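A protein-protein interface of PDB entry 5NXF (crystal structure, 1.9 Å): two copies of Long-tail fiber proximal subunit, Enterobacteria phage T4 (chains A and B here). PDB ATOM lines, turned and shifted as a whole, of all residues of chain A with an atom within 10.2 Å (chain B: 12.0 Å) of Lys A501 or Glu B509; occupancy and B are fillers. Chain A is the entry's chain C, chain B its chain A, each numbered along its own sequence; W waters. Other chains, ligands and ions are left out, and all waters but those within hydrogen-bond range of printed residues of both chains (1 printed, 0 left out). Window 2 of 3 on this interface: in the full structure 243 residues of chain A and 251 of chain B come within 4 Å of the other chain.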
ATOM      1  N   VAL A 495      30.785  14.175  11.127  1.00  0.00           N
ATOM      2  CA  VAL A 495      29.841  14.085  10.001  1.00  0.00           C
ATOM      3  C   VAL A 495      28.753  15.138  10.117  1.00  0.00           C
ATOM      4  O   VAL A 495      28.471  15.609  11.225  1.00  0.00           O
ATOM      5  CB  VAL A 495      29.202  12.688   9.833  1.00  0.00           C
ATOM      6  CG1 VAL A 495      30.269  11.602   9.838  1.00  0.00           C
ATOM      7  CG2 VAL A 495      28.145  12.412  10.894  1.00  0.00           C
ATOM      8  N   PRO A 496      28.152  15.528   8.967  1.00  0.00           N
ATOM      9  CA  PRO A 496      27.017  16.446   8.988  1.00  0.00           C
ATOM     10  C   PRO A 496      25.850  15.894   9.814  1.00  0.00           C
ATOM     11  O   PRO A 496      25.546  14.703   9.710  1.00  0.00           O
ATOM     12  CB  PRO A 496      26.618  16.553   7.502  1.00  0.00           C
ATOM     13  CG  PRO A 496      27.852  16.224   6.740  1.00  0.00           C
ATOM     14  CD  PRO A 496      28.551  15.198   7.582  1.00  0.00           C
ATOM     15  N   ASP A 497      25.250  16.762  10.632  1.00  0.00           N
ATOM     16  CA  ASP A 497      24.006  16.486  11.374  1.00  0.00           C
ATOM     17  C   ASP A 497      22.938  17.515  10.945  1.00  0.00           C
ATOM     18  O   ASP A 497      22.495  18.329  11.765  1.00  0.00           O
ATOM     19  CB  ASP A 497      24.263  16.570  12.894  1.00  0.00           C
ATOM     20  CG  ASP A 497      23.115  15.986  13.742  1.00  0.00           C
ATOM     21  OD1 ASP A 497      22.276  15.213  13.215  1.00  0.00           O
ATOM     22  OD2 ASP A 497      23.069  16.298  14.955  1.00  0.00           O
ATOM     23  N   PRO A 498      22.530  17.482   9.651  1.00  0.00           N
ATOM     24  CA  PRO A 498      21.689  18.550   9.080  1.00  0.00           C
ATOM     25  C   PRO A 498      20.333  18.726   9.771  1.00  0.00           C
ATOM     26  O   PRO A 498      19.860  19.859   9.888  1.00  0.00           O
ATOM     27  CB  PRO A 498      21.501  18.114   7.622  1.00  0.00           C
ATOM     28  CG  PRO A 498      21.669  16.637   7.644  1.00  0.00           C
ATOM     29  CD  PRO A 498      22.724  16.382   8.683  1.00  0.00           C
ATOM     30  N   VAL A 499      19.736  17.625  10.237  1.00  0.00           N
ATOM     31  CA  VAL A 499      18.468  17.674  10.979  1.00  0.00           C
ATOM     32  C   VAL A 499      18.556  18.511  12.279  1.00  0.00           C
ATOM     33  O   VAL A 499      17.553  19.107  12.688  1.00  0.00           O
ATOM     34  CB  VAL A 499      17.913  16.243  11.252  1.00  0.00           C
ATOM     35  CG1 VAL A 499      18.712  15.526  12.338  1.00  0.00           C
ATOM     36  CG2 VAL A 499      16.430  16.286  11.607  1.00  0.00           C
ATOM     37  N   ASN A 500      19.743  18.571  12.901  1.00  0.00           N
ATOM     38  CA  ASN A 500      19.977  19.371  14.119  1.00  0.00           C
ATOM     39  C   ASN A 500      20.839  20.633  13.919  1.00  0.00           C
ATOM     40  O   ASN A 500      21.415  21.146  14.885  1.00  0.00           O
ATOM     41  CB  ASN A 500      20.597  18.479  15.197  1.00  0.00           C
ATOM     42  CG  ASN A 500      19.636  17.418  15.692  1.00  0.00           C
ATOM     43  OD1 ASN A 500      19.797  16.225  15.416  1.00  0.00           O
ATOM     44  ND2 ASN A 500      18.616  17.850  16.419  1.00  0.00           N
ATOM     45  N   LYS A 501      20.905  21.148  12.687  1.00  0.00           N
ATOM     46  CA  LYS A 501      21.645  22.388  12.367  1.00  0.00           C
ATOM     47  C   LYS A 501      23.109  22.360  12.847  1.00  0.00           C
ATOM     48  O   LYS A 501      23.629  23.367  13.345  1.00  0.00           O
ATOM     49  CB  LYS A 501      20.920  23.633  12.942  1.00  0.00           C
ATOM     50  CG  LYS A 501      19.880  24.269  12.024  1.00  0.00           C
ATOM     51  CD  LYS A 501      19.432  25.643  12.537  1.00  0.00           C
ATOM     52  CE  LYS A 501      18.986  26.581  11.418  1.00  0.00           C
ATOM     53  NZ  LYS A 501      18.087  25.935  10.418  1.00  0.00           N
ATOM     54  N   THR A 502      23.776  21.216  12.695  1.00  0.00           N
ATOM     55  CA  THR A 502      25.142  21.077  13.210  1.00  0.00           C
ATOM     56  C   THR A 502      25.880  19.804  12.718  1.00  0.00           C
ATOM     57  O   THR A 502      25.611  19.301  11.621  1.00  0.00           O
ATOM     58  CB  THR A 502      25.143  21.177  14.757  1.00  0.00           C
ATOM     59  OG1 THR A 502      26.483  21.385  15.207  1.00  0.00           O
ATOM     60  CG2 THR A 502      24.493  19.922  15.412  1.00  0.00           C
ATOM     61  N   VAL A 503      26.812  19.306  13.528  1.00  0.00           N
ATOM     62  CA  VAL A 503      27.667  18.176  13.181  1.00  0.00           C
ATOM     63  C   VAL A 503      27.654  17.118  14.308  1.00  0.00           C
ATOM     64  O   VAL A 503      27.555  17.471  15.481  1.00  0.00           O
ATOM     65  CB  VAL A 503      29.087  18.744  12.924  1.00  0.00           C
ATOM     66  CG1 VAL A 503      30.175  17.817  13.393  1.00  0.00           C
ATOM     67  CG2 VAL A 503      29.274  19.114  11.455  1.00  0.00           C
ATOM     68  N   LYS A 504      27.747  15.836  13.939  1.00  0.00           N
ATOM     69  CA  LYS A 504      27.882  14.713  14.901  1.00  0.00           C
ATOM     70  C   LYS A 504      29.343  14.306  15.034  1.00  0.00           C
ATOM     71  O   LYS A 504      30.106  14.440  14.068  1.00  0.00           O
ATOM     72  CB  LYS A 504      27.120  13.467  14.428  1.00  0.00           C
ATOM     73  CG  LYS A 504      25.614  13.483  14.624  1.00  0.00           C
ATOM     74  CD  LYS A 504      24.967  12.193  14.120  1.00  0.00           C
ATOM     75  CE  LYS A 504      24.818  12.176  12.606  1.00  0.00           C
ATOM     76  NZ  LYS A 504      24.489  10.825  12.076  1.00  0.00           N
ATOM     77  N   ARG B 488      34.801  23.824   5.842  1.00  0.00           N
ATOM     78  CA  ARG B 488      33.395  23.518   5.845  1.00  0.00           C
ATOM     79  C   ARG B 488      33.188  22.016   5.855  1.00  0.00           C
ATOM     80  O   ARG B 488      33.792  21.306   5.051  1.00  0.00           O
ATOM     81  CB  ARG B 488      32.763  24.182   4.621  1.00  0.00           C
ATOM     82  CG  ARG B 488      31.283  24.407   4.781  1.00  0.00           C
ATOM     83  CD  ARG B 488      30.740  25.351   3.727  1.00  0.00           C
ATOM     84  NE  ARG B 488      29.308  25.135   3.533  1.00  0.00           N
ATOM     85  CZ  ARG B 488      28.533  25.879   2.744  1.00  0.00           C
ATOM     86  NH1 ARG B 488      29.030  26.932   2.071  1.00  0.00           N
ATOM     87  NH2 ARG B 488      27.244  25.572   2.650  1.00  0.00           N
ATOM     88  N   ILE B 489      32.356  21.529   6.781  1.00  0.00           N
ATOM     89  CA  ILE B 489      31.926  20.124   6.821  1.00  0.00           C
ATOM     90  C   ILE B 489      30.411  20.123   6.678  1.00  0.00           C
ATOM     91  O   ILE B 489      29.708  20.628   7.558  1.00  0.00           O
ATOM     92  CB  ILE B 489      32.264  19.419   8.155  1.00  0.00           C
ATOM     93  CG1 ILE B 489      33.710  19.671   8.552  1.00  0.00           C
ATOM     94  CG2 ILE B 489      32.002  17.916   8.036  1.00  0.00           C
ATOM     95  CD1 ILE B 489      34.092  18.982   9.852  1.00  0.00           C
ATOM     96  N   GLY B 490      29.913  19.534   5.593  1.00  0.00           N
ATOM     97  CA  GLY B 490      28.516  19.708   5.187  1.00  0.00           C
ATOM     98  C   GLY B 490      28.126  21.168   5.231  1.00  0.00           C
ATOM     99  O   GLY B 490      28.763  21.995   4.591  1.00  0.00           O
ATOM    100  N   ASN B 491      27.116  21.498   6.042  1.00  0.00           N
ATOM    101  CA  ASN B 491      26.657  22.885   6.177  1.00  0.00           C
ATOM    102  C   ASN B 491      27.193  23.606   7.426  1.00  0.00           C
ATOM    103  O   ASN B 491      26.684  24.661   7.785  1.00  0.00           O
ATOM    104  CB  ASN B 491      25.119  22.918   6.154  1.00  0.00           C
ATOM    105  CG  ASN B 491      24.573  24.162   5.485  1.00  0.00           C
ATOM    106  OD1 ASN B 491      24.901  24.446   4.330  1.00  0.00           O
ATOM    107  ND2 ASN B 491      23.740  24.911   6.204  1.00  0.00           N
ATOM    108  N   VAL B 492      28.229  23.048   8.067  1.00  0.00           N
ATOM    109  CA  VAL B 492      28.906  23.689   9.182  1.00  0.00           C
ATOM    110  C   VAL B 492      30.247  24.258   8.735  1.00  0.00           C
ATOM    111  O   VAL B 492      31.045  23.569   8.114  1.00  0.00           O
ATOM    112  CB  VAL B 492      29.114  22.708  10.348  1.00  0.00           C
ATOM    113  CG1 VAL B 492      29.965  23.340  11.442  1.00  0.00           C
ATOM    114  CG2 VAL B 492      27.756  22.277  10.901  1.00  0.00           C
ATOM    115  N   ARG B 493      30.470  25.513   9.104  1.00  0.00           N
ATOM    116  CA  ARG B 493      31.680  26.267   8.823  1.00  0.00           C
ATOM    117  C   ARG B 493      32.490  26.341  10.107  1.00  0.00           C
ATOM    118  O   ARG B 493      31.949  26.684  11.162  1.00  0.00           O
ATOM    119  CB  ARG B 493      31.261  27.671   8.400  1.00  0.00           C
ATOM    120  CG  ARG B 493      32.245  28.462   7.562  1.00  0.00           C
ATOM    121  CD  ARG B 493      31.491  29.543   6.786  1.00  0.00           C
ATOM    122  NE  ARG B 493      32.376  30.517   6.140  1.00  0.00           N
ATOM    123  CZ  ARG B 493      32.834  31.642   6.697  1.00  0.00           C
ATOM    124  NH1 ARG B 493      32.507  31.989   7.948  1.00  0.00           N
ATOM    125  NH2 ARG B 493      33.644  32.439   5.992  1.00  0.00           N
ATOM    126  N   ILE B 494      33.773  26.003  10.038  1.00  0.00           N
ATOM    127  CA  ILE B 494      34.687  26.193  11.155  1.00  0.00           C
ATOM    128  C   ILE B 494      35.668  27.310  10.780  1.00  0.00           C
ATOM    129  O   ILE B 494      36.427  27.179   9.799  1.00  0.00           O
ATOM    130  CB  ILE B 494      35.452  24.916  11.495  1.00  0.00           C
ATOM    131  CG1 ILE B 494      34.497  23.723  11.604  1.00  0.00           C
ATOM    132  CG2 ILE B 494      36.254  25.108  12.779  1.00  0.00           C
ATOM    133  CD1 ILE B 494      35.212  22.413  11.824  1.00  0.00           C
ATOM    134  N   VAL B 495      35.660  28.391  11.564  1.00  0.00           N
ATOM    135  CA  VAL B 495      36.516  29.559  11.314  1.00  0.00           C
ATOM    136  C   VAL B 495      37.403  29.904  12.524  1.00  0.00           C
ATOM    137  O   VAL B 495      37.089  29.503  13.645  1.00  0.00           O
ATOM    138  CB  VAL B 495      35.688  30.798  10.906  1.00  0.00           C
ATOM    139  CG1 VAL B 495      35.040  30.570   9.549  1.00  0.00           C
ATOM    140  CG2 VAL B 495      34.634  31.144  11.957  1.00  0.00           C
ATOM    141  N   LYS B 504      35.264  28.950  16.007  1.00  0.00           N
ATOM    142  CA  LYS B 504      33.802  28.963  16.011  1.00  0.00           C
ATOM    143  C   LYS B 504      33.269  27.936  15.023  1.00  0.00           C
ATOM    144  O   LYS B 504      33.728  27.876  13.887  1.00  0.00           O
ATOM    145  CB  LYS B 504      33.269  30.345  15.637  1.00  0.00           C
ATOM    146  CG  LYS B 504      33.413  31.383  16.736  1.00  0.00           C
ATOM    147  CD  LYS B 504      32.709  32.684  16.370  1.00  0.00           C
ATOM    148  CE  LYS B 504      33.474  33.905  16.856  1.00  0.00           C
ATOM    149  NZ  LYS B 504      32.813  35.184  16.476  1.00  0.00           N
ATOM    150  N   PHE B 505      32.309  27.134  15.477  1.00  0.00           N
ATOM    151  CA  PHE B 505      31.549  26.224  14.630  1.00  0.00           C
ATOM    152  C   PHE B 505      30.219  26.889  14.298  1.00  0.00           C
ATOM    153  O   PHE B 505      29.358  26.980  15.163  1.00  0.00           O
ATOM    154  CB  PHE B 505      31.263  24.926  15.360  1.00  0.00           C
ATOM    155  CG  PHE B 505      32.418  23.978  15.399  1.00  0.00           C
ATOM    156  CD1 PHE B 505      33.587  24.303  16.084  1.00  0.00           C
ATOM    157  CD2 PHE B 505      32.320  22.729  14.788  1.00  0.00           C
ATOM    158  CE1 PHE B 505      34.641  23.413  16.142  1.00  0.00           C
ATOM    159  CE2 PHE B 505      33.376  21.835  14.841  1.00  0.00           C
ATOM    160  CZ  PHE B 505      34.539  22.179  15.519  1.00  0.00           C
ATOM    161  N   GLU B 506      30.056  27.322  13.048  1.00  0.00           N
ATOM    162  CA  GLU B 506      28.919  28.134  12.607  1.00  0.00           C
ATOM    163  C   GLU B 506      28.065  27.410  11.559  1.00  0.00           C
ATOM    164  O   GLU B 506      28.527  27.172  10.432  1.00  0.00           O
ATOM    165  CB  GLU B 506      29.444  29.442  12.011  1.00  0.00           C
ATOM    166  CG  GLU B 506      30.370  30.214  12.944  1.00  0.00           C
ATOM    167  CD  GLU B 506      30.838  31.558  12.394  1.00  0.00           C
ATOM    168  OE1 GLU B 506      30.959  31.737  11.156  1.00  0.00           O
ATOM    169  OE2 GLU B 506      31.106  32.452  13.228  1.00  0.00           O
ATOM    170  N   TRP B 507      26.825  27.061  11.916  1.00  0.00           N
ATOM    171  CA  TRP B 507      25.887  26.488  10.941  1.00  0.00           C
ATOM    172  C   TRP B 507      25.638  27.537   9.867  1.00  0.00           C
ATOM    173  O   TRP B 507      25.374  28.678  10.183  1.00  0.00           O
ATOM    174  CB  TRP B 507      24.558  26.077  11.593  1.00  0.00           C
ATOM    175  CG  TRP B 507      23.480  25.638  10.604  1.00  0.00           C
ATOM    176  CD1 TRP B 507      22.456  26.403  10.129  1.00  0.00           C
ATOM    177  CD2 TRP B 507      23.340  24.352   9.976  1.00  0.00           C
ATOM    178  NE1 TRP B 507      21.679  25.676   9.253  1.00  0.00           N
ATOM    179  CE2 TRP B 507      22.198  24.416   9.141  1.00  0.00           C
ATOM    180  CE3 TRP B 507      24.064  23.155  10.037  1.00  0.00           C
ATOM    181  CZ2 TRP B 507      21.761  23.331   8.374  1.00  0.00           C
ATOM    182  CZ3 TRP B 507      23.618  22.066   9.288  1.00  0.00           C
ATOM    183  CH2 TRP B 507      22.478  22.168   8.460  1.00  0.00           C
ATOM    184  N   VAL B 508      25.764  27.149   8.607  1.00  0.00           N
ATOM    185  CA  VAL B 508      25.608  28.078   7.497  1.00  0.00           C
ATOM    186  C   VAL B 508      24.111  28.260   7.253  1.00  0.00           C
ATOM    187  O   VAL B 508      23.456  27.341   6.761  1.00  0.00           O
ATOM    188  CB  VAL B 508      26.264  27.540   6.210  1.00  0.00           C
ATOM    189  CG1 VAL B 508      25.950  28.460   5.020  1.00  0.00           C
ATOM    190  CG2 VAL B 508      27.770  27.356   6.407  1.00  0.00           C
ATOM    191  N   GLU B 509      23.587  29.441   7.598  1.00  0.00           N
ATOM    192  CA  GLU B 509      22.161  29.763   7.393  1.00  0.00           C
ATOM    193  C   GLU B 509      21.786  29.840   5.905  1.00  0.00           C
ATOM    194  O   GLU B 509      22.621  30.069   5.028  1.00  0.00           O
ATOM    195  CB  GLU B 509      21.783  31.078   8.100  1.00  0.00           C
ATOM    196  CG  GLU B 509      21.777  31.013   9.625  1.00  0.00           C
ATOM    197  CD  GLU B 509      20.554  30.305  10.217  1.00  0.00           C
ATOM    198  OE1 GLU B 509      19.875  29.525   9.512  1.00  0.00           O
ATOM    199  OE2 GLU B 509      20.271  30.520  11.417  1.00  0.00           O
ATOM    200  OXT GLU B 509      20.621  29.653   5.549  1.00  0.00           O
HETATM  201  O   HOH W   1      26.799  19.608   8.565  1.00  0.00           O
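The backbone NH of Asp A497 is in hydrogen-bond range of the backbone carbonyl oxygen of Thr A502, at 2.7 Å.
The guanidinium group (NE) of Arg B488 is in hydrogen-bond range of the backbone carbonyl oxygen (O) of Gly B490, at 3.4 Å.
Among the printed residues, pairs that only touch across the chains: Lys A501 with Trp B507 (3.1 Å), Thr A502 with Trp B507 (3.3 Å), Val A503 with Val B492 (3.6 Å), Thr A502 with Val B492 (3.6 Å), Lys A501 with Glu B509 (3.6 Å), Pro A498 with Trp B507 (3.8 Å) and Pro A496 with Gly B490 (3.9 Å).
Of the printed residues of chain B, Lys A501 touches Trp B507 (3.1 Å) and Glu B509 (3.6 Å).
Glu B509 touches just one residue of chain A: Lys A501.
Of chain B, only Trp B507 (3.8 Å) comes within 4 Å of Pro A498.
No residue of chain B comes within 4 Å of Asn A500.
Of chain A, only Pro A498 (3.8 Å), Lys A501 (3.1 Å) and Thr A502 (3.3 Å) come within 4 Å of Trp B507.
No residue of chain A comes within 4 Å of Val B508.
Printed residues of chain A within 4 Å of Gly B490: Pro A496 (3.9 Å).
Printed residues of chain B within 4 Å of Pro A496: Gly B490.
Of the printed residues of chain B, Val A503 touches Val B492.
Lys A504 touches none of the printed residues of chain B.
The nearest printed residue of chain B that does not touch Val A503 is Ile B489 (4.2 Å).
Of the 14 printed residues of chain B, 4 touch a printed residue of chain A.
Printed residues of chain B that touch a printed residue of chain A: Gly B490, Val B492, Trp B507 and Glu B509.
Hydrophobic or aromatic side chains of chain B within 4 Å of the printed part of chain A: Val B492 and Trp B507.
Among the printed residues, no Asp or Glu carboxylate lies within 4 Å of a Lys or Arg side-chain nitrogen of the other chain.
Positions printed for both chains: 495 and 504.
Of the 7 pairs that touch across the chains among the printed residues, none has its exchanged pair printed and touching as well.
Water W1 lies within hydrogen-bond range of the backbone NH (N) of Asn B491 (3.2 Å), the backbone carbonyl oxygen (O) of Ile B489 (3.2 Å) and the backbone carbonyl oxygen (O) of Thr A502 (3.3 Å).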
